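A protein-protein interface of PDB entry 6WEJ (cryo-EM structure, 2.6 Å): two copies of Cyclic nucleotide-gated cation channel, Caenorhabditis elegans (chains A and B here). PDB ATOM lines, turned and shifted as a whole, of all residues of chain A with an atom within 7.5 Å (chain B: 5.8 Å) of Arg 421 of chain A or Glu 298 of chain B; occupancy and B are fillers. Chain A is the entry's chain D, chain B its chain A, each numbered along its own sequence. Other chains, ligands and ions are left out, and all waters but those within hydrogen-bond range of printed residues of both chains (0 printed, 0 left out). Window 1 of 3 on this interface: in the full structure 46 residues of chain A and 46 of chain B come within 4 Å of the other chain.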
ATOM      1  N   ASN A 416      34.458  -2.319  23.264  1.00  0.00           N
ATOM      2  CA  ASN A 416      34.244  -2.205  24.701  1.00  0.00           C
ATOM      3  C   ASN A 416      32.769  -2.050  25.039  1.00  0.00           C
ATOM      4  O   ASN A 416      32.274  -2.683  25.975  1.00  0.00           O
ATOM      5  CB  ASN A 416      35.034  -1.029  25.269  1.00  0.00           C
ATOM      6  CG  ASN A 416      36.523  -1.232  25.179  1.00  0.00           C
ATOM      7  OD1 ASN A 416      37.288  -0.273  25.123  1.00  0.00           O
ATOM      8  ND2 ASN A 416      36.945  -2.486  25.154  1.00  0.00           N
ATOM      9  N   MET A 417      32.049  -1.214  24.296  1.00  0.00           N
ATOM     10  CA  MET A 417      30.673  -0.906  24.657  1.00  0.00           C
ATOM     11  C   MET A 417      29.696  -2.020  24.316  1.00  0.00           C
ATOM     12  O   MET A 417      28.519  -1.915  24.670  1.00  0.00           O
ATOM     13  CB  MET A 417      30.226   0.392  23.985  1.00  0.00           C
ATOM     14  CG  MET A 417      30.218   0.348  22.478  1.00  0.00           C
ATOM     15  SD  MET A 417      29.547   1.860  21.774  1.00  0.00           S
ATOM     16  CE  MET A 417      30.144   3.050  22.963  1.00  0.00           C
ATOM     17  N   SER A 418      30.143  -3.081  23.653  1.00  0.00           N
ATOM     18  CA  SER A 418      29.293  -4.224  23.347  1.00  0.00           C
ATOM     19  C   SER A 418      29.869  -5.511  23.922  1.00  0.00           C
ATOM     20  O   SER A 418      29.609  -6.596  23.405  1.00  0.00           O
ATOM     21  CB  SER A 418      29.090  -4.362  21.842  1.00  0.00           C
ATOM     22  OG  SER A 418      30.291  -4.744  21.202  1.00  0.00           O
ATOM     23  N   ALA A 419      30.651  -5.404  24.995  1.00  0.00           N
ATOM     24  CA  ALA A 419      31.279  -6.583  25.576  1.00  0.00           C
ATOM     25  C   ALA A 419      30.343  -7.305  26.532  1.00  0.00           C
ATOM     26  O   ALA A 419      30.334  -8.541  26.582  1.00  0.00           O
ATOM     27  CB  ALA A 419      32.567  -6.191  26.292  1.00  0.00           C
ATOM     28  N   ALA A 420      29.547  -6.555  27.297  1.00  0.00           N
ATOM     29  CA  ALA A 420      28.602  -7.179  28.215  1.00  0.00           C
ATOM     30  C   ALA A 420      27.515  -7.928  27.462  1.00  0.00           C
ATOM     31  O   ALA A 420      27.158  -9.052  27.830  1.00  0.00           O
ATOM     32  CB  ALA A 420      27.989  -6.124  29.129  1.00  0.00           C
ATOM     33  N   ARG A 421      26.969  -7.317  26.412  1.00  0.00           N
ATOM     34  CA  ARG A 421      25.979  -7.996  25.589  1.00  0.00           C
ATOM     35  C   ARG A 421      26.561  -9.253  24.961  1.00  0.00           C
ATOM     36  O   ARG A 421      25.897 -10.293  24.905  1.00  0.00           O
ATOM     37  CB  ARG A 421      25.462  -7.046  24.512  1.00  0.00           C
ATOM     38  CG  ARG A 421      24.601  -7.705  23.456  1.00  0.00           C
ATOM     39  CD  ARG A 421      23.243  -8.095  24.004  1.00  0.00           C
ATOM     40  NE  ARG A 421      22.548  -9.015  23.112  1.00  0.00           N
ATOM     41  CZ  ARG A 421      21.286  -9.397  23.270  1.00  0.00           C
ATOM     42  NH1 ARG A 421      20.737 -10.243  22.410  1.00  0.00           N
ATOM     43  NH2 ARG A 421      20.572  -8.933  24.282  1.00  0.00           N
ATOM     44  N   THR A 422      27.808  -9.181  24.497  1.00  0.00           N
ATOM     45  CA  THR A 422      28.448 -10.349  23.899  1.00  0.00           C
ATOM     46  C   THR A 422      28.610 -11.473  24.913  1.00  0.00           C
ATOM     47  O   THR A 422      28.339 -12.637  24.606  1.00  0.00           O
ATOM     48  CB  THR A 422      29.803  -9.959  23.316  1.00  0.00           C
ATOM     49  OG1 THR A 422      29.606  -9.111  22.180  1.00  0.00           O
ATOM     50  CG2 THR A 422      30.574 -11.191  22.895  1.00  0.00           C
ATOM     51  N   GLU A 423      29.059 -11.142  26.123  1.00  0.00           N
ATOM     52  CA  GLU A 423      29.245 -12.164  27.147  1.00  0.00           C
ATOM     53  C   GLU A 423      27.915 -12.788  27.554  1.00  0.00           C
ATOM     54  O   GLU A 423      27.814 -14.013  27.721  1.00  0.00           O
ATOM     55  CB  GLU A 423      29.958 -11.548  28.347  1.00  0.00           C
ATOM     56  CG  GLU A 423      29.608 -12.160  29.674  1.00  0.00           C
ATOM     57  CD  GLU A 423      30.342 -11.494  30.815  1.00  0.00           C
ATOM     58  OE1 GLU A 423      31.590 -11.525  30.815  1.00  0.00           O
ATOM     59  OE2 GLU A 423      29.674 -10.926  31.703  1.00  0.00           O
ATOM     60  N   PHE A 424      26.884 -11.959  27.718  1.00  0.00           N
ATOM     61  CA  PHE A 424      25.554 -12.477  28.009  1.00  0.00           C
ATOM     62  C   PHE A 424      25.077 -13.416  26.910  1.00  0.00           C
ATOM     63  O   PHE A 424      24.504 -14.475  27.190  1.00  0.00           O
ATOM     64  CB  PHE A 424      24.579 -11.315  28.187  1.00  0.00           C
ATOM     65  CG  PHE A 424      23.150 -11.738  28.293  1.00  0.00           C
ATOM     66  CD1 PHE A 424      22.629 -12.156  29.501  1.00  0.00           C
ATOM     67  CD2 PHE A 424      22.323 -11.710  27.185  1.00  0.00           C
ATOM     68  CE1 PHE A 424      21.316 -12.544  29.601  1.00  0.00           C
ATOM     69  CE2 PHE A 424      21.010 -12.103  27.281  1.00  0.00           C
ATOM     70  CZ  PHE A 424      20.507 -12.521  28.489  1.00  0.00           C
ATOM     71  N   GLN A 425      25.302 -13.044  25.650  1.00  0.00           N
ATOM     72  CA  GLN A 425      24.871 -13.892  24.550  1.00  0.00           C
ATOM     73  C   GLN A 425      25.640 -15.204  24.532  1.00  0.00           C
ATOM     74  O   GLN A 425      25.069 -16.257  24.237  1.00  0.00           O
ATOM     75  CB  GLN A 425      25.034 -13.156  23.225  1.00  0.00           C
ATOM     76  CG  GLN A 425      24.444 -13.894  22.039  1.00  0.00           C
ATOM     77  CD  GLN A 425      22.939 -14.018  22.127  1.00  0.00           C
ATOM     78  OE1 GLN A 425      22.376 -15.083  21.884  1.00  0.00           O
ATOM     79  NE2 GLN A 425      22.278 -12.921  22.473  1.00  0.00           N
ATOM     80  N   ASN A 426      26.934 -15.163  24.850  1.00  0.00           N
ATOM     81  CA  ASN A 426      27.717 -16.394  24.924  1.00  0.00           C
ATOM     82  C   ASN A 426      27.161 -17.331  25.986  1.00  0.00           C
ATOM     83  O   ASN A 426      27.014 -18.536  25.754  1.00  0.00           O
ATOM     84  CB  ASN A 426      29.182 -16.076  25.216  1.00  0.00           C
ATOM     85  CG  ASN A 426      29.861 -15.368  24.071  1.00  0.00           C
ATOM     86  OD1 ASN A 426      29.465 -15.507  22.917  1.00  0.00           O
ATOM     87  ND2 ASN A 426      30.899 -14.605  24.384  1.00  0.00           N
ATOM     88  N   LYS A 427      26.850 -16.793  27.167  1.00  0.00           N
ATOM     89  CA  LYS A 427      26.314 -17.641  28.230  1.00  0.00           C
ATOM     90  C   LYS A 427      24.945 -18.205  27.859  1.00  0.00           C
ATOM     91  O   LYS A 427      24.666 -19.387  28.100  1.00  0.00           O
ATOM     92  CB  LYS A 427      26.250 -16.859  29.540  1.00  0.00           C
ATOM     93  CG  LYS A 427      27.621 -16.469  30.061  1.00  0.00           C
ATOM     94  CD  LYS A 427      27.554 -15.764  31.403  1.00  0.00           C
ATOM     95  CE  LYS A 427      26.786 -14.457  31.309  1.00  0.00           C
ATOM     96  NZ  LYS A 427      26.812 -13.702  32.591  1.00  0.00           N
ATOM     97  N   MET A 428      24.088 -17.384  27.251  1.00  0.00           N
ATOM     98  CA  MET A 428      22.774 -17.866  26.843  1.00  0.00           C
ATOM     99  C   MET A 428      22.887 -18.944  25.771  1.00  0.00           C
ATOM    100  O   MET A 428      22.121 -19.913  25.771  1.00  0.00           O
ATOM    101  CB  MET A 428      21.925 -16.699  26.345  1.00  0.00           C
ATOM    102  CG  MET A 428      20.471 -17.046  26.119  1.00  0.00           C
ATOM    103  SD  MET A 428      19.801 -16.213  24.672  1.00  0.00           S
ATOM    104  CE  MET A 428      20.419 -14.555  24.924  1.00  0.00           C
ATOM    105  N   ASP A 453      16.204 -13.289  29.834  1.00  0.00           N
ATOM    106  CA  ASP A 453      15.884 -11.987  29.265  1.00  0.00           C
ATOM    107  C   ASP A 453      15.398 -11.021  30.336  1.00  0.00           C
ATOM    108  O   ASP A 453      15.678  -9.820  30.266  1.00  0.00           O
ATOM    109  CB  ASP A 453      14.840 -12.143  28.161  1.00  0.00           C
ATOM    110  CG  ASP A 453      15.311 -13.044  27.032  1.00  0.00           C
ATOM    111  OD1 ASP A 453      16.521 -13.037  26.721  1.00  0.00           O
ATOM    112  OD2 ASP A 453      14.468 -13.760  26.453  1.00  0.00           O
ATOM    113  N   TRP A 456      18.395  -9.744  32.150  1.00  0.00           N
ATOM    114  CA  TRP A 456      19.171  -8.916  31.242  1.00  0.00           C
ATOM    115  C   TRP A 456      18.509  -7.575  30.967  1.00  0.00           C
ATOM    116  O   TRP A 456      19.201  -6.619  30.606  1.00  0.00           O
ATOM    117  CB  TRP A 456      19.401  -9.644  29.919  1.00  0.00           C
ATOM    118  CG  TRP A 456      20.022  -8.786  28.874  1.00  0.00           C
ATOM    119  CD1 TRP A 456      19.443  -8.355  27.719  1.00  0.00           C
ATOM    120  CD2 TRP A 456      21.339  -8.225  28.896  1.00  0.00           C
ATOM    121  NE1 TRP A 456      20.321  -7.572  27.015  1.00  0.00           N
ATOM    122  CE2 TRP A 456      21.493  -7.477  27.717  1.00  0.00           C
ATOM    123  CE3 TRP A 456      22.405  -8.289  29.796  1.00  0.00           C
ATOM    124  CZ2 TRP A 456      22.665  -6.799  27.415  1.00  0.00           C
ATOM    125  CZ3 TRP A 456      23.568  -7.616  29.493  1.00  0.00           C
ATOM    126  CH2 TRP A 456      23.689  -6.880  28.315  1.00  0.00           C
ATOM    127  N   CYS B 293      11.925  -1.230  20.337  1.00  0.00           N
ATOM    128  CA  CYS B 293      11.623  -2.229  19.319  1.00  0.00           C
ATOM    129  C   CYS B 293      12.894  -2.852  18.767  1.00  0.00           C
ATOM    130  O   CYS B 293      12.952  -4.067  18.550  1.00  0.00           O
ATOM    131  CB  CYS B 293      10.802  -1.613  18.192  1.00  0.00           C
ATOM    132  SG  CYS B 293      10.539  -2.717  16.799  1.00  0.00           S
ATOM    133  N   LEU B 294      13.931  -2.048  18.545  1.00  0.00           N
ATOM    134  CA  LEU B 294      15.159  -2.600  17.984  1.00  0.00           C
ATOM    135  C   LEU B 294      15.842  -3.549  18.961  1.00  0.00           C
ATOM    136  O   LEU B 294      16.348  -4.601  18.558  1.00  0.00           O
ATOM    137  CB  LEU B 294      16.100  -1.477  17.565  1.00  0.00           C
ATOM    138  CG  LEU B 294      15.600  -0.670  16.371  1.00  0.00           C
ATOM    139  CD1 LEU B 294      16.612   0.378  15.977  1.00  0.00           C
ATOM    140  CD2 LEU B 294      15.297  -1.589  15.210  1.00  0.00           C
ATOM    141  N   GLU B 295      15.847  -3.218  20.253  1.00  0.00           N
ATOM    142  CA  GLU B 295      16.475  -4.127  21.208  1.00  0.00           C
ATOM    143  C   GLU B 295      15.629  -5.380  21.425  1.00  0.00           C
ATOM    144  O   GLU B 295      16.172  -6.490  21.502  1.00  0.00           O
ATOM    145  CB  GLU B 295      16.756  -3.410  22.528  1.00  0.00           C
ATOM    146  CG  GLU B 295      15.550  -2.823  23.212  1.00  0.00           C
ATOM    147  CD  GLU B 295      15.891  -2.160  24.531  1.00  0.00           C
ATOM    148  OE1 GLU B 295      15.353  -2.595  25.572  1.00  0.00           O
ATOM    149  OE2 GLU B 295      16.698  -1.208  24.530  1.00  0.00           O
ATOM    150  N   ARG B 296      14.303  -5.236  21.509  1.00  0.00           N
ATOM    151  CA  ARG B 296      13.448  -6.410  21.642  1.00  0.00           C
ATOM    152  C   ARG B 296      13.512  -7.291  20.405  1.00  0.00           C
ATOM    153  O   ARG B 296      13.226  -8.487  20.483  1.00  0.00           O
ATOM    154  CB  ARG B 296      12.003  -5.995  21.902  1.00  0.00           C
ATOM    155  CG  ARG B 296      11.757  -5.362  23.254  1.00  0.00           C
ATOM    156  CD  ARG B 296      10.462  -4.552  23.249  1.00  0.00           C
ATOM    157  NE  ARG B 296       9.269  -5.392  23.296  1.00  0.00           N
ATOM    158  CZ  ARG B 296       8.392  -5.385  24.295  1.00  0.00           C
ATOM    159  NH1 ARG B 296       8.567  -4.572  25.326  1.00  0.00           N
ATOM    160  NH2 ARG B 296       7.335  -6.184  24.260  1.00  0.00           N
ATOM    161  N   THR B 297      13.861  -6.722  19.255  1.00  0.00           N
ATOM    162  CA  THR B 297      14.048  -7.540  18.065  1.00  0.00           C
ATOM    163  C   THR B 297      15.420  -8.190  18.051  1.00  0.00           C
ATOM    164  O   THR B 297      15.572  -9.297  17.526  1.00  0.00           O
ATOM    165  CB  THR B 297      13.851  -6.689  16.813  1.00  0.00           C
ATOM    166  OG1 THR B 297      12.586  -6.026  16.887  1.00  0.00           O
ATOM    167  CG2 THR B 297      13.872  -7.553  15.578  1.00  0.00           C
ATOM    168  N   GLU B 298      16.422  -7.524  18.620  1.00  0.00           N
ATOM    169  CA  GLU B 298      17.739  -8.139  18.721  1.00  0.00           C
ATOM    170  C   GLU B 298      17.716  -9.336  19.658  1.00  0.00           C
ATOM    171  O   GLU B 298      18.349 -10.357  19.375  1.00  0.00           O
ATOM    172  CB  GLU B 298      18.763  -7.110  19.188  1.00  0.00           C
ATOM    173  CG  GLU B 298      20.149  -7.674  19.389  1.00  0.00           C
ATOM    174  CD  GLU B 298      21.159  -6.610  19.749  1.00  0.00           C
ATOM    175  OE1 GLU B 298      21.929  -6.194  18.858  1.00  0.00           O
ATOM    176  OE2 GLU B 298      21.180  -6.178  20.919  1.00  0.00           O
ATOM    177  N   THR B 299      16.993  -9.235  20.775  1.00  0.00           N
ATOM    178  CA  THR B 299      16.945 -10.367  21.697  1.00  0.00           C
ATOM    179  C   THR B 299      16.165 -11.538  21.115  1.00  0.00           C
ATOM    180  O   THR B 299      16.488 -12.694  21.402  1.00  0.00           O
ATOM    181  CB  THR B 299      16.337  -9.957  23.035  1.00  0.00           C
ATOM    182  OG1 THR B 299      14.943  -9.680  22.868  1.00  0.00           O
ATOM    183  CG2 THR B 299      17.039  -8.733  23.583  1.00  0.00           C
ATOM    184  N   ARG B 300      15.148 -11.269  20.303  1.00  0.00           N
ATOM    185  CA  ARG B 300      14.389 -12.331  19.661  1.00  0.00           C
ATOM    186  C   ARG B 300      15.068 -12.891  18.423  1.00  0.00           C
ATOM    187  O   ARG B 300      14.656 -13.949  17.938  1.00  0.00           O
ATOM    188  CB  ARG B 300      13.005 -11.829  19.261  1.00  0.00           C
ATOM    189  CG  ARG B 300      12.141 -11.390  20.406  1.00  0.00           C
ATOM    190  CD  ARG B 300      10.760 -11.064  19.908  1.00  0.00           C
ATOM    191  NE  ARG B 300       9.834 -10.873  21.011  1.00  0.00           N
ATOM    192  CZ  ARG B 300       8.546 -11.175  20.952  1.00  0.00           C
ATOM    193  NH1 ARG B 300       8.037 -11.690  19.843  1.00  0.00           N
ATOM    194  NH2 ARG B 300       7.771 -10.972  22.006  1.00  0.00           N
ATOM    195  N   SER B 301      16.081 -12.215  17.896  1.00  0.00           N
ATOM    196  CA  SER B 301      16.659 -12.593  16.616  1.00  0.00           C
ATOM    197  C   SER B 301      17.539 -13.826  16.754  1.00  0.00           C
ATOM    198  O   SER B 301      18.332 -13.945  17.691  1.00  0.00           O
ATOM    199  CB  SER B 301      17.476 -11.440  16.039  1.00  0.00           C
ATOM    200  OG  SER B 301      17.865 -11.720  14.707  1.00  0.00           O
ATOM    201  N   SER B 302      17.394 -14.744  15.805  1.00  0.00           N
ATOM    202  CA  SER B 302      18.238 -15.927  15.743  1.00  0.00           C
ATOM    203  C   SER B 302      19.640 -15.622  15.240  1.00  0.00           C
ATOM    204  O   SER B 302      20.448 -16.546  15.113  1.00  0.00           O
ATOM    205  CB  SER B 302      17.583 -16.980  14.851  1.00  0.00           C
ATOM    206  OG  SER B 302      17.250 -16.431  13.590  1.00  0.00           O
ATOM    207  N   PRO B 304      21.936 -12.450  16.248  1.00  0.00           N
ATOM    208  CA  PRO B 304      22.068 -11.113  16.853  1.00  0.00           C
ATOM    209  C   PRO B 304      23.217 -10.291  16.294  1.00  0.00           C
ATOM    210  O   PRO B 304      23.087  -9.067  16.176  1.00  0.00           O
ATOM    211  CB  PRO B 304      22.266 -11.430  18.341  1.00  0.00           C
ATOM    212  CG  PRO B 304      22.854 -12.793  18.353  1.00  0.00           C
ATOM    213  CD  PRO B 304      22.219 -13.525  17.212  1.00  0.00           C
ATOM    214  N   PHE B 307      22.097  -9.065  12.919  1.00  0.00           N
ATOM    215  CA  PHE B 307      21.065  -8.050  13.083  1.00  0.00           C
ATOM    216  C   PHE B 307      21.656  -6.733  13.557  1.00  0.00           C
ATOM    217  O   PHE B 307      21.203  -5.660  13.144  1.00  0.00           O
ATOM    218  CB  PHE B 307      19.995  -8.540  14.054  1.00  0.00           C
ATOM    219  CG  PHE B 307      18.829  -7.617  14.178  1.00  0.00           C
ATOM    220  CD1 PHE B 307      17.813  -7.639  13.242  1.00  0.00           C
ATOM    221  CD2 PHE B 307      18.747  -6.721  15.227  1.00  0.00           C
ATOM    222  CE1 PHE B 307      16.739  -6.784  13.352  1.00  0.00           C
ATOM    223  CE2 PHE B 307      17.676  -5.864  15.340  1.00  0.00           C
ATOM    224  CZ  PHE B 307      16.672  -5.896  14.401  1.00  0.00           C
ATOM    225  N   ARG B 308      22.662  -6.790  14.426  1.00  0.00           N
ATOM    226  CA  ARG B 308      23.328  -5.569  14.869  1.00  0.00           C
ATOM    227  C   ARG B 308      23.985  -4.856  13.694  1.00  0.00           C
ATOM    228  O   ARG B 308      23.817  -3.641  13.508  1.00  0.00           O
ATOM    229  CB  ARG B 308      24.348  -5.913  15.952  1.00  0.00           C
ATOM    230  CG  ARG B 308      25.078  -4.732  16.558  1.00  0.00           C
ATOM    231  CD  ARG B 308      25.405  -4.989  18.022  1.00  0.00           C
ATOM    232  NE  ARG B 308      25.818  -6.371  18.261  1.00  0.00           N
ATOM    233  CZ  ARG B 308      26.147  -6.861  19.454  1.00  0.00           C
ATOM    234  NH1 ARG B 308      26.506  -8.130  19.575  1.00  0.00           N
ATOM    235  NH2 ARG B 308      26.117  -6.085  20.528  1.00  0.00           N
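Of the 13 printed residues of chain B, 4 touch a printed residue of chain A. Hydrophobic or aromatic side chains of chain B within 4 Å of the printed part of chain A: Pro 304. Among the printed residues, 5 pairs touch across the chains. Among the printed residues, Asp or Glu carboxylates within 4 Å of a Lys or Arg side-chain nitrogen of the other chain: Arg 421 of chain A with Glu 298 of chain B (3.8 Å).
OE2 of Glu 298 of chain B is in salt-bridge range of NE of Arg 421 of chain A (3.8 Å).
O of Arg 296 of chain B is in hydrogen-bond range of OG1 of Thr 299 of chain B. The side-chain carboxylate (OE1) of Glu 298 of chain B is in salt-bridge range of the guanidinium group (NE) of Arg 308 of chain B. O of Ser 418 of chain A lies within hydrogen-bond range of OG1 of Thr 422 of chain A, at 2.8 Å. NE2 of Gln 425 of chain A lies close to NH1 of Arg 421 of chain A.
No position is printed for both chains.
Among the printed residues, merely in contact across the chains: Ser 418 of chain A with Arg 308 of chain B (3.7 Å), Arg 421 of chain A with Thr 299 of chain B (3.6 Å), Arg 421 of chain A with Arg 308 of chain B (3.7 Å) and Gln 425 of chain A with Pro 304 of chain B (3.97 Å).
Of the printed residues of chain B, Arg 421 of chain A touches Glu 298 (3.8 Å), Thr 299 (3.6 Å) and Arg 308 (3.7 Å). Printed residues of chain B within 4 Å of Ser 418 of chain A: Arg 308. Of the printed residues of chain A, Arg 308 of chain B touches Ser 418 (3.7 Å) and Arg 421 (3.7 Å). Printed residues of chain B within 4 Å of Gln 425 of chain A: Pro 304. Of the printed residues of chain A, Pro 304 of chain B touches Gln 425. Printed residues of chain A within 4 Å of Thr 299 of chain B: Arg 421 (3.6 Å). Leu 294 of chain B touches none of the printed residues of chain A. The nearest residue of chain B that does not touch Arg 421 of chain A is Pro 304 of chain B (4.5 Å). The nearest residue of chain A that does not touch Glu 298 of chain B is Gln 425 of chain A (5.6 Å).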
